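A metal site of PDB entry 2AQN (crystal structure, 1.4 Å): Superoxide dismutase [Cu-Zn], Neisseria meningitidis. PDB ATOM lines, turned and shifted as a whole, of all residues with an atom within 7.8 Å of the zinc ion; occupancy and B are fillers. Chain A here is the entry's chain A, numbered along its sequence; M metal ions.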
ATOM      1  N   PHE A  56      22.405  -6.487 -32.538  1.00  0.00           N
ATOM      2  CA  PHE A  56      21.412  -7.409 -33.102  1.00  0.00           C
ATOM      3  C   PHE A  56      21.428  -8.660 -32.276  1.00  0.00           C
ATOM      4  O   PHE A  56      22.410  -9.408 -32.246  1.00  0.00           O
ATOM      5  CB  PHE A  56      21.830  -7.657 -34.517  1.00  0.00           C
ATOM      6  CG  PHE A  56      20.904  -8.251 -35.517  1.00  0.00           C
ATOM      7  CD1 PHE A  56      19.554  -7.944 -35.532  1.00  0.00           C
ATOM      8  CD2 PHE A  56      21.374  -9.158 -36.469  1.00  0.00           C
ATOM      9  CE1 PHE A  56      18.708  -8.458 -36.515  1.00  0.00           C
ATOM     10  CE2 PHE A  56      20.555  -9.655 -37.473  1.00  0.00           C
ATOM     11  CZ  PHE A  56      19.210  -9.301 -37.466  1.00  0.00           C
ATOM     12  N   HIS A  57      20.365  -8.921 -31.506  1.00  0.00           N
ATOM     13  CA  HIS A  57      20.390 -10.038 -30.558  1.00  0.00           C
ATOM     14  C   HIS A  57      19.015 -10.717 -30.466  1.00  0.00           C
ATOM     15  O   HIS A  57      17.999 -10.052 -30.649  1.00  0.00           O
ATOM     16  CB  HIS A  57      20.763  -9.619 -29.157  1.00  0.00           C
ATOM     17  CG  HIS A  57      21.732  -8.489 -29.017  1.00  0.00           C
ATOM     18  ND1 HIS A  57      21.376  -7.239 -28.530  1.00  0.00           N
ATOM     19  CD2 HIS A  57      23.033  -8.402 -29.411  1.00  0.00           C
ATOM     20  CE1 HIS A  57      22.452  -6.454 -28.576  1.00  0.00           C
ATOM     21  NE2 HIS A  57      23.446  -7.133 -29.104  1.00  0.00           N
ATOM     22  N   ILE A  58      19.013 -11.987 -30.172  1.00  0.00           N
ATOM     23  CA  ILE A  58      17.788 -12.625 -29.708  1.00  0.00           C
ATOM     24  C   ILE A  58      17.539 -12.281 -28.246  1.00  0.00           C
ATOM     25  O   ILE A  58      18.455 -12.510 -27.457  1.00  0.00           O
ATOM     26  CB  ILE A  58      17.902 -14.153 -29.890  1.00  0.00           C
ATOM     27  CG1 ILE A  58      18.377 -14.569 -31.251  1.00  0.00           C
ATOM     28  CG2 ILE A  58      16.556 -14.813 -29.522  1.00  0.00           C
ATOM     29  CD1 ILE A  58      17.486 -14.221 -32.419  1.00  0.00           C
ATOM     30  N   HIS A  59      16.329 -11.808 -27.931  1.00  0.00           N
ATOM     31  CA  HIS A  59      15.920 -11.544 -26.561  1.00  0.00           C
ATOM     32  C   HIS A  59      14.951 -12.629 -26.098  1.00  0.00           C
ATOM     33  O   HIS A  59      14.353 -13.357 -26.880  1.00  0.00           O
ATOM     34  CB  HIS A  59      15.309 -10.141 -26.369  1.00  0.00           C
ATOM     35  CG  HIS A  59      16.362  -9.066 -26.442  1.00  0.00           C
ATOM     36  ND1 HIS A  59      16.532  -8.138 -25.449  1.00  0.00           N
ATOM     37  CD2 HIS A  59      17.329  -8.762 -27.360  1.00  0.00           C
ATOM     38  CE1 HIS A  59      17.542  -7.324 -25.752  1.00  0.00           C
ATOM     39  NE2 HIS A  59      18.029  -7.676 -26.909  1.00  0.00           N
ATOM     40  N   GLY A  81      15.689  -9.685 -21.408  1.00  0.00           N
ATOM     41  CA  GLY A  81      17.127  -9.489 -21.668  1.00  0.00           C
ATOM     42  C   GLY A  81      17.565 -10.375 -22.838  1.00  0.00           C
ATOM     43  O   GLY A  81      16.764 -11.034 -23.517  1.00  0.00           O
ATOM     44  N   HIS A  82      18.887 -10.378 -23.084  1.00  0.00           N
ATOM     45  CA  HIS A  82      19.453 -11.267 -24.077  1.00  0.00           C
ATOM     46  C   HIS A  82      19.153 -12.706 -23.719  1.00  0.00           C
ATOM     47  O   HIS A  82      19.290 -13.118 -22.571  1.00  0.00           O
ATOM     48  CB  HIS A  82      20.975 -11.073 -24.230  1.00  0.00           C
ATOM     49  CG  HIS A  82      21.357  -9.706 -24.703  1.00  0.00           C
ATOM     50  ND1 HIS A  82      22.609  -9.471 -25.160  1.00  0.00           N
ATOM     51  CD2 HIS A  82      20.679  -8.540 -24.802  1.00  0.00           C
ATOM     52  CE1 HIS A  82      22.682  -8.180 -25.517  1.00  0.00           C
ATOM     53  NE2 HIS A  82      21.512  -7.583 -25.314  1.00  0.00           N
ATOM     54  N   TRP A  83      18.763 -13.454 -24.754  1.00  0.00           N
ATOM     55  CA  TRP A  83      18.445 -14.878 -24.542  1.00  0.00           C
ATOM     56  C   TRP A  83      19.673 -15.621 -24.082  1.00  0.00           C
ATOM     57  O   TRP A  83      20.694 -15.619 -24.809  1.00  0.00           O
ATOM     58  CB  TRP A  83      17.799 -15.456 -25.809  1.00  0.00           C
ATOM     59  CG  TRP A  83      17.303 -16.872 -25.624  1.00  0.00           C
ATOM     60  CD1 TRP A  83      16.549 -17.346 -24.579  1.00  0.00           C
ATOM     61  CD2 TRP A  83      17.531 -17.961 -26.497  1.00  0.00           C
ATOM     62  NE1 TRP A  83      16.305 -18.685 -24.768  1.00  0.00           N
ATOM     63  CE2 TRP A  83      16.887 -19.089 -25.938  1.00  0.00           C
ATOM     64  CE3 TRP A  83      18.203 -18.114 -27.690  1.00  0.00           C
ATOM     65  CZ2 TRP A  83      16.889 -20.349 -26.508  1.00  0.00           C
ATOM     66  CZ3 TRP A  83      18.209 -19.377 -28.274  1.00  0.00           C
ATOM     67  CH2 TRP A  83      17.560 -20.451 -27.676  1.00  0.00           C
ATOM     68  N   ASP A  84      19.563 -16.252 -22.908  1.00  0.00           N
ATOM     69  CA  ASP A  84      20.722 -16.891 -22.263  1.00  0.00           C
ATOM     70  C   ASP A  84      20.339 -18.184 -21.576  1.00  0.00           C
ATOM     71  O   ASP A  84      20.497 -18.343 -20.372  1.00  0.00           O
ATOM     72  CB  ASP A  84      21.303 -15.887 -21.275  1.00  0.00           C
ATOM     73  CG  ASP A  84      22.624 -16.288 -20.679  1.00  0.00           C
ATOM     74  OD1 ASP A  84      23.353 -17.095 -21.285  1.00  0.00           O
ATOM     75  OD2 ASP A  84      22.947 -15.791 -19.564  1.00  0.00           O
ATOM     76  N   LYS A  89      25.576 -15.483 -18.690  1.00  0.00           N
ATOM     77  CA  LYS A  89      25.541 -14.262 -17.897  1.00  0.00           C
ATOM     78  C   LYS A  89      26.639 -13.308 -18.320  1.00  0.00           C
ATOM     79  O   LYS A  89      27.151 -12.616 -17.461  1.00  0.00           O
ATOM     80  CB  LYS A  89      25.684 -14.549 -16.390  1.00  0.00           C
ATOM     81  CG  LYS A  89      24.576 -15.405 -15.834  1.00  0.00           C
ATOM     82  CD  LYS A  89      24.911 -16.243 -14.585  1.00  0.00           C
ATOM     83  CE  LYS A  89      24.163 -17.546 -14.524  1.00  0.00           C
ATOM     84  NZ  LYS A  89      24.856 -18.845 -14.239  1.00  0.00           N
ATOM     85  N   GLN A  90      26.934 -13.240 -19.605  1.00  0.00           N
ATOM     86  CA  GLN A  90      27.959 -12.364 -20.139  1.00  0.00           C
ATOM     87  C   GLN A  90      27.607 -12.103 -21.599  1.00  0.00           C
ATOM     88  O   GLN A  90      27.221 -13.085 -22.253  1.00  0.00           O
ATOM     89  CB  GLN A  90      29.344 -12.965 -20.013  1.00  0.00           C
ATOM     90  CG  GLN A  90      30.451 -12.588 -20.944  1.00  0.00           C
ATOM     91  CD  GLN A  90      31.713 -13.315 -20.451  1.00  0.00           C
ATOM     92  OE1 GLN A  90      32.098 -13.063 -19.316  1.00  0.00           O
ATOM     93  NE2 GLN A  90      32.315 -14.179 -21.227  1.00  0.00           N
ATOM     94  N   HIS A  91      27.732 -10.889 -22.047  1.00  0.00           N
ATOM     95  CA  HIS A  91      27.603 -10.569 -23.462  1.00  0.00           C
ATOM     96  C   HIS A  91      28.928 -10.781 -24.196  1.00  0.00           C
ATOM     97  O   HIS A  91      29.990 -10.486 -23.681  1.00  0.00           O
ATOM     98  CB  HIS A  91      27.154  -9.113 -23.628  1.00  0.00           C
ATOM     99  CG  HIS A  91      26.838  -8.790 -25.055  1.00  0.00           C
ATOM    100  ND1 HIS A  91      25.770  -9.285 -25.745  1.00  0.00           N
ATOM    101  CD2 HIS A  91      27.548  -7.975 -25.898  1.00  0.00           C
ATOM    102  CE1 HIS A  91      25.818  -8.784 -26.981  1.00  0.00           C
ATOM    103  NE2 HIS A  91      26.866  -7.997 -27.093  1.00  0.00           N
ATOM    104  N   GLY A  92      28.879 -11.346 -25.414  1.00  0.00           N
ATOM    105  CA  GLY A  92      30.083 -11.682 -26.134  1.00  0.00           C
ATOM    106  C   GLY A  92      29.845 -11.739 -27.630  1.00  0.00           C
ATOM    107  O   GLY A  92      28.938 -11.169 -28.220  1.00  0.00           O
ATOM    108  N   TYR A  93      30.714 -12.417 -28.348  1.00  0.00           N
ATOM    109  CA  TYR A  93      30.848 -12.642 -29.713  1.00  0.00           C
ATOM    110  C   TYR A  93      29.897 -13.766 -30.168  1.00  0.00           C
ATOM    111  O   TYR A  93      29.593 -14.663 -29.403  1.00  0.00           O
ATOM    112  CB  TYR A  93      32.250 -13.050 -30.227  1.00  0.00           C
ATOM    113  CG  TYR A  93      33.253 -11.928 -30.048  1.00  0.00           C
ATOM    114  CD1 TYR A  93      33.360 -10.921 -30.997  1.00  0.00           C
ATOM    115  CD2 TYR A  93      34.075 -11.884 -28.937  1.00  0.00           C
ATOM    116  CE1 TYR A  93      34.263  -9.881 -30.882  1.00  0.00           C
ATOM    117  CE2 TYR A  93      34.992 -10.839 -28.806  1.00  0.00           C
ATOM    118  CZ  TYR A  93      35.078  -9.855 -29.762  1.00  0.00           C
ATOM    119  OH  TYR A  93      35.977  -8.823 -29.625  1.00  0.00           O
ATOM    120  N   ALA A  99      29.197 -16.844 -24.057  1.00  0.00           N
ATOM    121  CA  ALA A  99      28.423 -15.654 -24.241  1.00  0.00           C
ATOM    122  C   ALA A  99      26.954 -16.029 -24.343  1.00  0.00           C
ATOM    123  O   ALA A  99      26.643 -17.161 -24.640  1.00  0.00           O
ATOM    124  CB  ALA A  99      28.856 -14.930 -25.511  1.00  0.00           C
ATOM    125  N   HIS A 100      26.078 -15.063 -24.150  1.00  0.00           N
ATOM    126  CA  HIS A 100      24.638 -15.273 -24.382  1.00  0.00           C
ATOM    127  C   HIS A 100      24.373 -15.976 -25.716  1.00  0.00           C
ATOM    128  O   HIS A 100      24.950 -15.526 -26.728  1.00  0.00           O
ATOM    129  CB  HIS A 100      23.915 -13.952 -24.419  1.00  0.00           C
ATOM    130  CG  HIS A 100      24.057 -12.975 -23.309  1.00  0.00           C
ATOM    131  ND1 HIS A 100      24.224 -11.641 -23.483  1.00  0.00           N
ATOM    132  CD2 HIS A 100      23.968 -13.165 -21.961  1.00  0.00           C
ATOM    133  CE1 HIS A 100      24.265 -11.049 -22.288  1.00  0.00           C
ATOM    134  NE2 HIS A 100      24.117 -11.956 -21.339  1.00  0.00           N
ATOM    135  N   LEU A 101      23.558 -17.021 -25.714  1.00  0.00           N
ATOM    136  CA  LEU A 101      23.266 -17.679 -26.988  1.00  0.00           C
ATOM    137  C   LEU A 101      22.571 -16.743 -27.982  1.00  0.00           C
ATOM    138  O   LEU A 101      22.633 -16.996 -29.195  1.00  0.00           O
ATOM    139  CB  LEU A 101      22.398 -18.915 -26.738  1.00  0.00           C
ATOM    140  CG  LEU A 101      22.309 -19.951 -27.832  1.00  0.00           C
ATOM    141  CD1 LEU A 101      23.713 -20.529 -28.142  1.00  0.00           C
ATOM    142  CD2 LEU A 101      21.353 -21.088 -27.503  1.00  0.00           C
ATOM    143  N   GLY A 102      21.873 -15.713 -27.527  1.00  0.00           N
ATOM    144  CA  GLY A 102      21.239 -14.777 -28.448  1.00  0.00           C
ATOM    145  C   GLY A 102      22.162 -13.767 -29.068  1.00  0.00           C
ATOM    146  O   GLY A 102      21.651 -12.902 -29.793  1.00  0.00           O
ATOM    147  N   ASP A 103      23.459 -13.788 -28.851  1.00  0.00           N
ATOM    148  CA  ASP A 103      24.385 -12.738 -29.383  1.00  0.00           C
ATOM    149  C   ASP A 103      24.685 -13.007 -30.849  1.00  0.00           C
ATOM    150  O   ASP A 103      25.352 -13.997 -31.165  1.00  0.00           O
ATOM    151  CB  ASP A 103      25.657 -12.682 -28.529  1.00  0.00           C
ATOM    152  CG  ASP A 103      25.399 -12.203 -27.096  1.00  0.00           C
ATOM    153  OD1 ASP A 103      24.269 -11.654 -26.845  1.00  0.00           O
ATOM    154  OD2 ASP A 103      26.285 -12.371 -26.231  1.00  0.00           O
ATOM    155  N   LEU A 104      24.116 -12.161 -31.745  1.00  0.00           N
ATOM    156  CA  LEU A 104      24.291 -12.321 -33.180  1.00  0.00           C
ATOM    157  C   LEU A 104      25.369 -11.359 -33.683  1.00  0.00           C
ATOM    158  O   LEU A 104      25.700 -10.408 -32.953  1.00  0.00           O
ATOM    159  CB  LEU A 104      22.977 -12.053 -33.917  1.00  0.00           C
ATOM    160  CG  LEU A 104      21.702 -12.728 -33.405  1.00  0.00           C
ATOM    161  CD1 LEU A 104      20.479 -12.196 -34.139  1.00  0.00           C
ATOM    162  CD2 LEU A 104      21.833 -14.241 -33.534  1.00  0.00           C
ATOM    163  N   ARG A 123      26.387 -20.587 -33.319  1.00  0.00           N
ATOM    164  CA  ARG A 123      25.986 -21.386 -32.153  1.00  0.00           C
ATOM    165  C   ARG A 123      24.513 -21.716 -32.139  1.00  0.00           C
ATOM    166  O   ARG A 123      24.057 -22.508 -31.297  1.00  0.00           O
ATOM    167  CB  ARG A 123      26.352 -20.609 -30.871  1.00  0.00           C
ATOM    168  CG  ARG A 123      27.855 -20.508 -30.765  1.00  0.00           C
ATOM    169  CD  ARG A 123      28.260 -19.792 -29.484  1.00  0.00           C
ATOM    170  NE  ARG A 123      27.949 -18.398 -29.312  1.00  0.00           N
ATOM    171  CZ  ARG A 123      27.329 -17.798 -28.323  1.00  0.00           C
ATOM    172  NH1 ARG A 123      26.791 -18.417 -27.283  1.00  0.00           N
ATOM    173  NH2 ARG A 123      27.181 -16.463 -28.347  1.00  0.00           N
ATOM    174  N   ASP A 142      27.716  -2.789 -31.373  1.00  0.00           N
ATOM    175  CA  ASP A 142      28.006  -3.969 -30.545  1.00  0.00           C
ATOM    176  C   ASP A 142      29.499  -4.292 -30.592  1.00  0.00           C
ATOM    177  O   ASP A 142      30.000  -4.778 -31.608  1.00  0.00           O
ATOM    178  CB  ASP A 142      27.191  -5.171 -30.984  1.00  0.00           C
ATOM    179  CG  ASP A 142      27.097  -6.316 -29.997  1.00  0.00           C
ATOM    180  OD1 ASP A 142      27.884  -6.330 -29.044  1.00  0.00           O
ATOM    181  OD2 ASP A 142      26.204  -7.233 -30.141  1.00  0.00           O
ATOM    182  N   HIS A 144      30.669  -6.507 -28.554  1.00  0.00           N
ATOM    183  CA  HIS A 144      30.687  -7.915 -28.146  1.00  0.00           C
ATOM    184  C   HIS A 144      31.368  -8.088 -26.786  1.00  0.00           C
ATOM    185  O   HIS A 144      32.042  -9.073 -26.488  1.00  0.00           O
ATOM    186  CB  HIS A 144      31.301  -8.827 -29.191  1.00  0.00           C
ATOM    187  CG  HIS A 144      30.510  -8.816 -30.461  1.00  0.00           C
ATOM    188  ND1 HIS A 144      29.221  -9.322 -30.548  1.00  0.00           N
ATOM    189  CD2 HIS A 144      30.800  -8.356 -31.686  1.00  0.00           C
ATOM    190  CE1 HIS A 144      28.772  -9.154 -31.804  1.00  0.00           C
ATOM    191  NE2 HIS A 144      29.719  -8.562 -32.534  1.00  0.00           N
ATOM    192  N   SER A 145      31.153  -7.126 -25.907  1.00  0.00           N
ATOM    193  CA  SER A 145      31.641  -7.146 -24.539  1.00  0.00           C
ATOM    194  C   SER A 145      30.703  -6.351 -23.609  1.00  0.00           C
ATOM    195  O   SER A 145      29.882  -5.578 -24.073  1.00  0.00           O
ATOM    196  CB  SER A 145      33.043  -6.532 -24.604  1.00  0.00           C
ATOM    197  OG  SER A 145      33.584  -6.522 -23.357  1.00  0.00           O
ATOM    198  N   ASP A 146      30.861  -6.564 -22.305  1.00  0.00           N
ATOM    199  CA  ASP A 146      30.147  -5.723 -21.357  1.00  0.00           C
ATOM    200  C   ASP A 146      31.018  -4.602 -20.830  1.00  0.00           C
ATOM    201  O   ASP A 146      30.681  -3.950 -19.826  1.00  0.00           O
ATOM    202  CB  ASP A 146      29.637  -6.582 -20.188  1.00  0.00           C
ATOM    203  CG  ASP A 146      28.550  -7.551 -20.571  1.00  0.00           C
ATOM    204  OD1 ASP A 146      27.476  -7.092 -21.043  1.00  0.00           O
ATOM    205  OD2 ASP A 146      28.722  -8.811 -20.403  1.00  0.00           O
ATOM    206  N   LEU A 151      26.325  -4.951 -22.471  1.00  0.00           N
ATOM    207  CA  LEU A 151      25.598  -5.470 -23.627  1.00  0.00           C
ATOM    208  C   LEU A 151      26.055  -4.860 -24.927  1.00  0.00           C
ATOM    209  O   LEU A 151      25.281  -4.626 -25.862  1.00  0.00           O
ATOM    210  CB  LEU A 151      24.101  -5.278 -23.385  1.00  0.00           C
ATOM    211  CG  LEU A 151      23.589  -5.923 -22.068  1.00  0.00           C
ATOM    212  CD1 LEU A 151      22.235  -5.373 -21.675  1.00  0.00           C
ATOM    213  CD2 LEU A 151      23.517  -7.444 -22.181  1.00  0.00           C
ATOM    214  N   GLY A 152      27.388  -4.681 -24.993  1.00  0.00           N
ATOM    215  CA  GLY A 152      28.067  -4.285 -26.193  1.00  0.00           C
ATOM    216  C   GLY A 152      27.857  -2.857 -26.595  1.00  0.00           C
ATOM    217  O   GLY A 152      28.287  -2.470 -27.679  1.00  0.00           O
HETATM  218 ZN    ZN M   1      24.295 -10.608 -25.228  1.00  0.00          ZN
HETATM  219 CU    CU M   2      19.604  -6.856 -27.708  1.00  0.00          CU
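The zinc ion is bound by the side-chain carboxylate of Asp 103 (1.9 Å), a ring nitrogen (ND1) of His 100 (2.0 Å), a ring nitrogen (ND1) of His 82 (2.0 Å) and a ring nitrogen (ND1) of His 91 (2.0 Å). Slightly farther from the zinc ion lies OD2 of Asp 103 (2.8 Å).
The side-chain carboxylate of Asp 103 is in hydrogen-bond range of the backbone NH of Gly 92 (2.9 Å). O of Gln 90 lies within hydrogen-bond range of N of His 100 (3.0 Å). The backbone carbonyl oxygen of His 100 lies within hydrogen-bond range of the guanidinium group of Arg 123, 2.9 Å away. A ring nitrogen (NE2) of His 82 sits close to a ring nitrogen (ND1) of His 57 (3.2 Å). A ring nitrogen (NE2) of His 91 lies within hydrogen-bond range of the side-chain carboxylate (OD1) of Asp 142. The side-chain carboxylate of Asp 146 lies within hydrogen-bond range of the backbone NH of His 91, 2.8 Å away.
Of the 26 residues printed, 4 come within 4 Å of the zinc ion.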
